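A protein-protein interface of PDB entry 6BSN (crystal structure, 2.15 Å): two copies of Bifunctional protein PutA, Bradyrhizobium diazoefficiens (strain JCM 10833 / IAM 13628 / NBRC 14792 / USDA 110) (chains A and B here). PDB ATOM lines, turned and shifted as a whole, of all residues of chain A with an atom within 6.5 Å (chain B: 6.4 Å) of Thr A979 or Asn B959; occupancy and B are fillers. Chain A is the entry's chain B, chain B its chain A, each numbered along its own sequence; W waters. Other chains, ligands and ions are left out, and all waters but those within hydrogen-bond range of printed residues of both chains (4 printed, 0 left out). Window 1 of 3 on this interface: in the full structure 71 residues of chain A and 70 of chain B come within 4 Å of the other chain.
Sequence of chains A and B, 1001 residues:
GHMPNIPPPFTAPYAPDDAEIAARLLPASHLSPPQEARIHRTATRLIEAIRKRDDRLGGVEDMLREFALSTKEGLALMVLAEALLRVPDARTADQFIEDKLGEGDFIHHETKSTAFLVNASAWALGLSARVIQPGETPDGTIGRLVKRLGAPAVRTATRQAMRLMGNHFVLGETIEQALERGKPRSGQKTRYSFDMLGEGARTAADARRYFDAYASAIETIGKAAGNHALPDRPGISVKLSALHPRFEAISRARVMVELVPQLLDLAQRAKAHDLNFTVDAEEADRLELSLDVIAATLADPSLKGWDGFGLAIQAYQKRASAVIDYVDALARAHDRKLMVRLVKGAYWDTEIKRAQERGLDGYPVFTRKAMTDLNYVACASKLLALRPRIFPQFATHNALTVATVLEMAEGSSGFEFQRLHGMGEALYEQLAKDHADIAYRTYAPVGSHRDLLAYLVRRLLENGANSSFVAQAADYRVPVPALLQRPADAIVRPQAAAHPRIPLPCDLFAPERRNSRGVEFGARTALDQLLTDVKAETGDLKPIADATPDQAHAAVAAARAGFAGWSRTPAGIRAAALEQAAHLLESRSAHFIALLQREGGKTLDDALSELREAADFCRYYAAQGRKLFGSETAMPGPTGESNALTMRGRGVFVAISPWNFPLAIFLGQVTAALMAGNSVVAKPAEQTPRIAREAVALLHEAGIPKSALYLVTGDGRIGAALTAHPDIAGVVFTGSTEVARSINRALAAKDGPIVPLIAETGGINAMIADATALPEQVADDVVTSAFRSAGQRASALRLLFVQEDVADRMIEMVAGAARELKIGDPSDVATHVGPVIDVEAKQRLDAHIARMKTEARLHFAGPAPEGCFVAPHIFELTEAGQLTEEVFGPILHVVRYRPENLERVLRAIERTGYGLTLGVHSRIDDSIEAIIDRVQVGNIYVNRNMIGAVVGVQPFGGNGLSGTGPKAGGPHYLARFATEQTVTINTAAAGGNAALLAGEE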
ATOM      1  N   THR A 646      20.468  12.608   0.594  1.00  0.00           N
ATOM      2  CA  THR A 646      20.097  11.958   1.839  1.00  0.00           C
ATOM      3  C   THR A 646      20.760  10.594   1.874  1.00  0.00           C
ATOM      4  O   THR A 646      21.369  10.145   0.901  1.00  0.00           O
ATOM      5  CB  THR A 646      18.569  11.786   1.981  1.00  0.00           C
ATOM      6  OG1 THR A 646      18.014  11.285   0.758  1.00  0.00           O
ATOM      7  CG2 THR A 646      17.882  13.105   2.332  1.00  0.00           C
ATOM      8  N   MET A 647      20.612   9.924   3.004  1.00  0.00           N
ATOM      9  CA  MET A 647      21.076   8.559   3.145  1.00  0.00           C
ATOM     10  C   MET A 647      19.977   7.793   3.853  1.00  0.00           C
ATOM     11  O   MET A 647      19.322   8.327   4.749  1.00  0.00           O
ATOM     12  CB  MET A 647      22.397   8.479   3.935  1.00  0.00           C
ATOM     13  CG  MET A 647      23.625   8.928   3.150  1.00  0.00           C
ATOM     14  SD  MET A 647      25.172   8.542   3.993  1.00  0.00           S
ATOM     15  CE  MET A 647      25.264   9.920   5.136  1.00  0.00           C
ATOM     16  N   ARG A 648      19.747   6.560   3.433  1.00  0.00           N
ATOM     17  CA  ARG A 648      18.677   5.778   4.032  1.00  0.00           C
ATOM     18  C   ARG A 648      19.133   4.336   4.225  1.00  0.00           C
ATOM     19  O   ARG A 648      20.114   3.885   3.625  1.00  0.00           O
ATOM     20  CB  ARG A 648      17.406   5.840   3.175  1.00  0.00           C
ATOM     21  CG  ARG A 648      17.613   5.549   1.691  1.00  0.00           C
ATOM     22  CD  ARG A 648      16.394   6.036   0.895  1.00  0.00           C
ATOM     23  NE  ARG A 648      15.201   5.300   1.282  1.00  0.00           N
ATOM     24  CZ  ARG A 648      13.951   5.650   0.978  1.00  0.00           C
ATOM     25  NH1 ARG A 648      12.935   4.894   1.393  1.00  0.00           N
ATOM     26  NH2 ARG A 648      13.705   6.741   0.253  1.00  0.00           N
ATOM     27  N   GLY A 649      18.405   3.617   5.080  1.00  0.00           N
ATOM     28  CA  GLY A 649      18.707   2.222   5.357  1.00  0.00           C
ATOM     29  C   GLY A 649      18.776   1.373   4.106  1.00  0.00           C
ATOM     30  O   GLY A 649      18.160   1.715   3.099  1.00  0.00           O
ATOM     31  N   ARG A 650      19.554   0.292   4.139  1.00  0.00           N
ATOM     32  CA  ARG A 650      19.708  -0.572   2.977  1.00  0.00           C
ATOM     33  C   ARG A 650      18.709  -1.712   2.960  1.00  0.00           C
ATOM     34  O   ARG A 650      18.251  -2.096   1.884  1.00  0.00           O
ATOM     35  CB  ARG A 650      21.122  -1.165   2.929  1.00  0.00           C
ATOM     36  CG  ARG A 650      22.225  -0.168   2.685  1.00  0.00           C
ATOM     37  CD  ARG A 650      23.599  -0.858   2.550  1.00  0.00           C
ATOM     38  NE  ARG A 650      24.502  -0.031   1.769  1.00  0.00           N
ATOM     39  CZ  ARG A 650      24.609  -0.089   0.447  1.00  0.00           C
ATOM     40  NH1 ARG A 650      23.896  -0.957  -0.238  1.00  0.00           N
ATOM     41  NH2 ARG A 650      25.440   0.720  -0.190  1.00  0.00           N
ATOM     42  N   ALA A 676      21.428   3.400  11.171  1.00  0.00           N
ATOM     43  CA  ALA A 676      21.385   3.728   9.754  1.00  0.00           C
ATOM     44  C   ALA A 676      20.065   3.349   9.094  1.00  0.00           C
ATOM     45  O   ALA A 676      19.938   3.523   7.877  1.00  0.00           O
ATOM     46  CB  ALA A 676      22.533   3.047   9.027  1.00  0.00           C
ATOM     47  N   PRO A 753      21.913  -8.478  -5.678  1.00  0.00           N
ATOM     48  CA  PRO A 753      22.788  -7.308  -5.551  1.00  0.00           C
ATOM     49  C   PRO A 753      24.102  -7.634  -4.851  1.00  0.00           C
ATOM     50  O   PRO A 753      24.178  -8.512  -3.986  1.00  0.00           O
ATOM     51  CB  PRO A 753      21.957  -6.333  -4.715  1.00  0.00           C
ATOM     52  CG  PRO A 753      20.505  -6.753  -4.983  1.00  0.00           C
ATOM     53  CD  PRO A 753      20.573  -8.252  -5.102  1.00  0.00           C
ATOM     54  N   ALA A 975      27.825   5.577   7.567  1.00  0.00           N
ATOM     55  CA  ALA A 975      27.480   5.742   6.156  1.00  0.00           C
ATOM     56  C   ALA A 975      27.550   4.423   5.402  1.00  0.00           C
ATOM     57  O   ALA A 975      26.776   4.204   4.464  1.00  0.00           O
ATOM     58  CB  ALA A 975      28.389   6.774   5.488  1.00  0.00           C
ATOM     59  N   ARG A 976      28.470   3.537   5.789  1.00  0.00           N
ATOM     60  CA  ARG A 976      28.635   2.281   5.070  1.00  0.00           C
ATOM     61  C   ARG A 976      27.413   1.381   5.175  1.00  0.00           C
ATOM     62  O   ARG A 976      27.236   0.511   4.321  1.00  0.00           O
ATOM     63  CB  ARG A 976      29.885   1.545   5.570  1.00  0.00           C
ATOM     64  CG  ARG A 976      30.316   0.390   4.683  1.00  0.00           C
ATOM     65  CD  ARG A 976      30.941   0.922   3.391  1.00  0.00           C
ATOM     66  NE  ARG A 976      31.457  -0.208   2.653  1.00  0.00           N
ATOM     67  CZ  ARG A 976      30.808  -0.826   1.675  1.00  0.00           C
ATOM     68  NH1 ARG A 976      29.617  -0.397   1.287  1.00  0.00           N
ATOM     69  NH2 ARG A 976      31.355  -1.877   1.084  1.00  0.00           N
ATOM     70  N   PHE A 977      26.594   1.543   6.216  1.00  0.00           N
ATOM     71  CA  PHE A 977      25.359   0.789   6.392  1.00  0.00           C
ATOM     72  C   PHE A 977      24.182   1.412   5.656  1.00  0.00           C
ATOM     73  O   PHE A 977      23.048   0.927   5.796  1.00  0.00           O
ATOM     74  CB  PHE A 977      25.005   0.673   7.878  1.00  0.00           C
ATOM     75  CG  PHE A 977      26.041  -0.051   8.701  1.00  0.00           C
ATOM     76  CD1 PHE A 977      27.206   0.600   9.100  1.00  0.00           C
ATOM     77  CD2 PHE A 977      25.840  -1.360   9.104  1.00  0.00           C
ATOM     78  CE1 PHE A 977      28.168  -0.052   9.860  1.00  0.00           C
ATOM     79  CE2 PHE A 977      26.795  -2.025   9.884  1.00  0.00           C
ATOM     80  CZ  PHE A 977      27.964  -1.364  10.259  1.00  0.00           C
ATOM     81  N   ALA A 978      24.416   2.470   4.887  1.00  0.00           N
ATOM     82  CA  ALA A 978      23.338   3.209   4.245  1.00  0.00           C
ATOM     83  C   ALA A 978      23.584   3.282   2.748  1.00  0.00           C
ATOM     84  O   ALA A 978      24.651   2.923   2.248  1.00  0.00           O
ATOM     85  CB  ALA A 978      23.198   4.621   4.830  1.00  0.00           C
ATOM     86  N   THR A 979      22.567   3.737   2.020  1.00  0.00           N
ATOM     87  CA  THR A 979      22.734   4.042   0.609  1.00  0.00           C
ATOM     88  C   THR A 979      22.280   5.478   0.392  1.00  0.00           C
ATOM     89  O   THR A 979      21.496   6.003   1.176  1.00  0.00           O
ATOM     90  CB  THR A 979      21.969   3.038  -0.283  1.00  0.00           C
ATOM     91  OG1 THR A 979      22.387   3.211  -1.634  1.00  0.00           O
ATOM     92  CG2 THR A 979      20.470   3.236  -0.188  1.00  0.00           C
ATOM     93  N   GLU A 980      22.833   6.130  -0.628  1.00  0.00           N
ATOM     94  CA  GLU A 980      22.564   7.541  -0.875  1.00  0.00           C
ATOM     95  C   GLU A 980      21.337   7.734  -1.763  1.00  0.00           C
ATOM     96  O   GLU A 980      21.060   6.932  -2.649  1.00  0.00           O
ATOM     97  CB  GLU A 980      23.752   8.205  -1.558  1.00  0.00           C
ATOM     98  CG  GLU A 980      25.055   8.283  -0.769  1.00  0.00           C
ATOM     99  CD  GLU A 980      26.238   8.525  -1.705  1.00  0.00           C
ATOM    100  OE1 GLU A 980      26.768   7.542  -2.253  1.00  0.00           O
ATOM    101  OE2 GLU A 980      26.615   9.697  -1.924  1.00  0.00           O
ATOM    102  N   GLN A 981      20.667   8.870  -1.598  1.00  0.00           N
ATOM    103  CA  GLN A 981      19.548   9.192  -2.472  1.00  0.00           C
ATOM    104  C   GLN A 981      19.595  10.666  -2.840  1.00  0.00           C
ATOM    105  O   GLN A 981      19.686  11.530  -1.963  1.00  0.00           O
ATOM    106  CB  GLN A 981      18.212   8.833  -1.805  1.00  0.00           C
ATOM    107  CG  GLN A 981      16.985   9.152  -2.644  1.00  0.00           C
ATOM    108  CD  GLN A 981      15.797   8.338  -2.207  1.00  0.00           C
ATOM    109  OE1 GLN A 981      15.156   8.665  -1.224  1.00  0.00           O
ATOM    110  NE2 GLN A 981      15.507   7.250  -2.935  1.00  0.00           N
ATOM    111  N   GLY B 762      23.800   0.071 -14.299  1.00  0.00           N
ATOM    112  CA  GLY B 762      22.610   0.318 -15.084  1.00  0.00           C
ATOM    113  C   GLY B 762      21.315   0.269 -14.290  1.00  0.00           C
ATOM    114  O   GLY B 762      21.281   0.302 -13.057  1.00  0.00           O
ATOM    115  N   GLY B 913      14.481  -5.184  -9.275  1.00  0.00           N
ATOM    116  CA  GLY B 913      15.719  -5.226  -8.527  1.00  0.00           C
ATOM    117  C   GLY B 913      16.677  -4.081  -8.807  1.00  0.00           C
ATOM    118  O   GLY B 913      17.662  -3.919  -8.072  1.00  0.00           O
ATOM    119  N   TYR B 914      16.430  -3.283  -9.840  1.00  0.00           N
ATOM    120  CA  TYR B 914      17.283  -2.148 -10.143  1.00  0.00           C
ATOM    121  C   TYR B 914      16.832  -0.917  -9.353  1.00  0.00           C
ATOM    122  O   TYR B 914      15.749  -0.883  -8.771  1.00  0.00           O
ATOM    123  CB  TYR B 914      17.267  -1.857 -11.648  1.00  0.00           C
ATOM    124  CG  TYR B 914      18.032  -2.866 -12.467  1.00  0.00           C
ATOM    125  CD1 TYR B 914      19.416  -2.762 -12.624  1.00  0.00           C
ATOM    126  CD2 TYR B 914      17.377  -3.923 -13.099  1.00  0.00           C
ATOM    127  CE1 TYR B 914      20.122  -3.668 -13.382  1.00  0.00           C
ATOM    128  CE2 TYR B 914      18.083  -4.849 -13.862  1.00  0.00           C
ATOM    129  CZ  TYR B 914      19.448  -4.719 -14.004  1.00  0.00           C
ATOM    130  OH  TYR B 914      20.155  -5.639 -14.763  1.00  0.00           O
ATOM    131  N   GLY B 915      17.684   0.104  -9.329  1.00  0.00           N
ATOM    132  CA  GLY B 915      17.314   1.329  -8.650  1.00  0.00           C
ATOM    133  C   GLY B 915      18.234   2.487  -8.951  1.00  0.00           C
ATOM    134  O   GLY B 915      18.880   3.026  -8.047  1.00  0.00           O
ATOM    135  N   LEU B 916      18.308   2.881 -10.219  1.00  0.00           N
ATOM    136  CA  LEU B 916      19.248   3.919 -10.632  1.00  0.00           C
ATOM    137  C   LEU B 916      18.532   5.264 -10.770  1.00  0.00           C
ATOM    138  O   LEU B 916      18.717   6.143  -9.929  1.00  0.00           O
ATOM    139  CB  LEU B 916      19.953   3.523 -11.935  1.00  0.00           C
ATOM    140  CG  LEU B 916      21.167   4.369 -12.339  1.00  0.00           C
ATOM    141  CD1 LEU B 916      22.125   4.614 -11.142  1.00  0.00           C
ATOM    142  CD2 LEU B 916      21.920   3.720 -13.478  1.00  0.00           C
ATOM    143  N   GLN B 936      13.616   3.143  -3.300  1.00  0.00           N
ATOM    144  CA  GLN B 936      15.005   3.267  -2.856  1.00  0.00           C
ATOM    145  C   GLN B 936      15.936   3.822  -3.934  1.00  0.00           C
ATOM    146  O   GLN B 936      17.138   4.003  -3.685  1.00  0.00           O
ATOM    147  CB  GLN B 936      15.508   1.905  -2.372  1.00  0.00           C
ATOM    148  CG  GLN B 936      15.210   1.642  -0.921  1.00  0.00           C
ATOM    149  CD  GLN B 936      15.874   0.377  -0.426  1.00  0.00           C
ATOM    150  OE1 GLN B 936      15.551  -0.717  -0.878  1.00  0.00           O
ATOM    151  NE2 GLN B 936      16.833   0.525   0.486  1.00  0.00           N
ATOM    152  N   VAL B 937      15.389   4.111  -5.113  1.00  0.00           N
ATOM    153  CA  VAL B 937      16.123   4.542  -6.290  1.00  0.00           C
ATOM    154  C   VAL B 937      17.113   5.657  -5.968  1.00  0.00           C
ATOM    155  O   VAL B 937      16.809   6.565  -5.192  1.00  0.00           O
ATOM    156  CB  VAL B 937      15.072   4.979  -7.327  1.00  0.00           C
ATOM    157  CG1 VAL B 937      15.717   5.433  -8.604  1.00  0.00           C
ATOM    158  CG2 VAL B 937      14.045   3.807  -7.554  1.00  0.00           C
ATOM    159  N   GLY B 938      18.294   5.602  -6.604  1.00  0.00           N
ATOM    160  CA  GLY B 938      19.385   6.501  -6.235  1.00  0.00           C
ATOM    161  C   GLY B 938      19.197   7.941  -6.697  1.00  0.00           C
ATOM    162  O   GLY B 938      19.642   8.874  -6.030  1.00  0.00           O
ATOM    163  N   GLY B 957      24.191   7.595  -8.864  1.00  0.00           N
ATOM    164  CA  GLY B 957      24.368   6.188  -8.552  1.00  0.00           C
ATOM    165  C   GLY B 957      23.249   5.678  -7.668  1.00  0.00           C
ATOM    166  O   GLY B 957      22.566   6.423  -6.970  1.00  0.00           O
ATOM    167  N   GLY B 958      23.050   4.366  -7.708  1.00  0.00           N
ATOM    168  CA  GLY B 958      21.925   3.757  -7.024  1.00  0.00           C
ATOM    169  C   GLY B 958      22.301   2.478  -6.298  1.00  0.00           C
ATOM    170  O   GLY B 958      23.431   2.328  -5.835  1.00  0.00           O
ATOM    171  N   ASN B 959      21.370   1.538  -6.203  1.00  0.00           N
ATOM    172  CA  ASN B 959      21.521   0.399  -5.314  1.00  0.00           C
ATOM    173  C   ASN B 959      20.882  -0.819  -5.976  1.00  0.00           C
ATOM    174  O   ASN B 959      20.470  -0.776  -7.144  1.00  0.00           O
ATOM    175  CB  ASN B 959      20.881   0.726  -3.961  1.00  0.00           C
ATOM    176  CG  ASN B 959      19.456   1.253  -4.125  1.00  0.00           C
ATOM    177  OD1 ASN B 959      18.572   0.510  -4.512  1.00  0.00           O
ATOM    178  ND2 ASN B 959      19.242   2.536  -3.847  1.00  0.00           N
ATOM    179  N   GLY B 960      20.780  -1.907  -5.215  1.00  0.00           N
ATOM    180  CA  GLY B 960      20.291  -3.152  -5.783  1.00  0.00           C
ATOM    181  C   GLY B 960      21.139  -3.546  -6.973  1.00  0.00           C
ATOM    182  O   GLY B 960      22.355  -3.331  -6.985  1.00  0.00           O
ATOM    183  N   LEU B 961      20.487  -4.060  -8.024  1.00  0.00           N
ATOM    184  CA  LEU B 961      21.215  -4.452  -9.225  1.00  0.00           C
ATOM    185  C   LEU B 961      21.795  -3.257  -9.973  1.00  0.00           C
ATOM    186  O   LEU B 961      22.507  -3.456 -10.960  1.00  0.00           O
ATOM    187  CB  LEU B 961      20.300  -5.272 -10.152  1.00  0.00           C
ATOM    188  CG  LEU B 961      19.681  -6.539  -9.547  1.00  0.00           C
ATOM    189  CD1 LEU B 961      18.747  -7.296 -10.550  1.00  0.00           C
ATOM    190  CD2 LEU B 961      20.764  -7.466  -9.033  1.00  0.00           C
ATOM    191  N   SER B 962      21.526  -2.025  -9.539  1.00  0.00           N
ATOM    192  CA  SER B 962      22.178  -0.875 -10.158  1.00  0.00           C
ATOM    193  C   SER B 962      23.583  -0.590  -9.614  1.00  0.00           C
ATOM    194  O   SER B 962      24.294   0.225 -10.207  1.00  0.00           O
ATOM    195  CB  SER B 962      21.292   0.359 -10.015  1.00  0.00           C
ATOM    196  OG  SER B 962      20.115   0.140 -10.774  1.00  0.00           O
ATOM    197  N   GLY B 963      24.015  -1.237  -8.535  1.00  0.00           N
ATOM    198  CA  GLY B 963      25.409  -1.143  -8.147  1.00  0.00           C
ATOM    199  C   GLY B 963      25.583  -0.956  -6.654  1.00  0.00           C
ATOM    200  O   GLY B 963      24.655  -1.133  -5.872  1.00  0.00           O
ATOM    201  N   THR B 964      26.806  -0.569  -6.261  1.00  0.00           N
ATOM    202  CA  THR B 964      27.232  -0.591  -4.868  1.00  0.00           C
ATOM    203  C   THR B 964      27.253   0.780  -4.220  1.00  0.00           C
ATOM    204  O   THR B 964      27.296   0.861  -2.991  1.00  0.00           O
ATOM    205  CB  THR B 964      28.662  -1.156  -4.738  1.00  0.00           C
ATOM    206  OG1 THR B 964      29.554  -0.362  -5.538  1.00  0.00           O
ATOM    207  CG2 THR B 964      28.738  -2.619  -5.192  1.00  0.00           C
ATOM    208  N   GLY B 965      27.269   1.852  -5.000  1.00  0.00           N
ATOM    209  CA  GLY B 965      27.713   3.111  -4.456  1.00  0.00           C
ATOM    210  C   GLY B 965      29.214   3.039  -4.194  1.00  0.00           C
ATOM    211  O   GLY B 965      29.864   2.028  -4.486  1.00  0.00           O
ATOM    212  N   LYS B 967      28.025   7.219  -4.647  1.00  0.00           N
ATOM    213  CA  LYS B 967      27.611   7.978  -5.822  1.00  0.00           C
ATOM    214  C   LYS B 967      28.782   8.743  -6.426  1.00  0.00           C
ATOM    215  O   LYS B 967      29.487   9.480  -5.728  1.00  0.00           O
ATOM    216  CB  LYS B 967      26.493   8.967  -5.455  1.00  0.00           C
ATOM    217  CG  LYS B 967      25.108   8.349  -5.215  1.00  0.00           C
ATOM    218  CD  LYS B 967      24.140   9.413  -4.681  1.00  0.00           C
ATOM    219  CE  LYS B 967      22.673   9.008  -4.849  1.00  0.00           C
ATOM    220  NZ  LYS B 967      22.244   9.072  -6.281  1.00  0.00           N
HETATM  221  O   HOH W   1      26.523   2.932  -1.243  1.00  0.00           O
HETATM  222  O   HOH W   2      28.892  10.390  -3.234  1.00  0.00           O
HETATM  223  O   HOH W   3      24.119   1.885  -3.124  1.00  0.00           O
HETATM  224  O   HOH W   4      15.767   2.972   2.682  1.00  0.00           O
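The side-chain amide nitrogen (NE2) of Gln B936 sits at hydrogen-bond distance from the backbone carbonyl oxygen (O) of Arg A650 (3.3 Å).
N of Lys B967 sits at hydrogen-bond distance from OE1 of Glu A980 (2.7 Å).
O of Thr B964 lies within hydrogen-bond range of NH2 of Arg A650 (3.4 Å).
NE2 of Gln A981 sits at hydrogen-bond distance from O of Val B937, at 2.7 Å.
NE2 of Gln B936 sits at hydrogen-bond distance from O of Gly A649, 3.2 Å away.
O of Leu B916 is in hydrogen-bond range of N of Gly B938 (3.4 Å).
O of Gly B915 sits at hydrogen-bond distance from N of Asn B959 (3.4 Å).
O of Gly B915 is in hydrogen-bond range of N of Gly B938, 3.0 Å away.
The backbone carbonyl oxygen (O) of Ala A978 lies within hydrogen-bond range of the guanidinium group (NE) of Arg A650.
The backbone carbonyl oxygen (O) of Gly B957 lies within hydrogen-bond range of the side-chain amino group (NZ) of Lys B967, 2.8 Å away.
O of Gly B913 sits at hydrogen-bond distance from N of Leu B961 (2.8 Å).
Gly B960 touches Pro A753 (C to CB, 3.7 Å).
Pro A753 touches Leu B961 (N to CD2, 3.7 Å).
OG1 of Thr A979 touches CB of Asn B959 (3.7 Å).
O of Glu A980 touches CA of Gly B938, at 3.98 Å.
NE2 of Gln A981 touches C of Gln B936, at 3.6 Å.
Gln A981 touches Gly B938.
Lys B967 touches Gln A981.
Printed residues of chain B within 4 Å of Pro A753: Gly B960 and Leu B961.
Thr A979 touches just one residue of chain B: Asn B959.
Gly B762 touches none of the printed residues of chain A.
Printed residues of chain A within 4 Å of Gln B936: Gly A649, Arg A650 and Gln A981.
Asn B959 touches one residue of chain A.
The nearest printed residue of chain A that does not touch Leu B961 is Arg A650 (9.0 Å).
Of the 14 printed residues of chain A, 6 touch a printed residue of chain B.
Along chain A the printed residues that touch a printed residue of chain B span positions 649 to 981.
Of the 18 printed residues of chain B, 8 touch a printed residue of chain A.
Hydrophobic or aromatic side chains of chain B that line the printed part of chain A: Leu B961.
Among the printed residues, 12 pairs touch across the chains.
Among the printed residues, no Asp or Glu carboxylate lies within 4 Å of a Lys or Arg side-chain nitrogen of the other chain.
No position is printed for both chains.
Of the 12 pairs that touch across the chains among the printed residues, none has its exchanged pair printed and touching as well.
Water W3 lies within hydrogen-bond range of OG1 of Thr A979 (2.6 Å), O of Gly B958 (2.8 Å), O of Thr B964 (3.3 Å) and NH2 of Arg A650 (3.4 Å).
Water W1 lies within hydrogen-bond range of NH2 of Arg A650 (2.7 Å) and O of Thr B964 (2.8 Å).
Water W2 bridges OE2 of Glu A980 (2.7 Å) and O of Lys B967 (2.7 Å).
Water W4 lies within hydrogen-bond range of O of Gly A649 (2.7 Å), NE of Arg A648 (2.8 Å) and NE2 of Gln B936 (3.5 Å).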
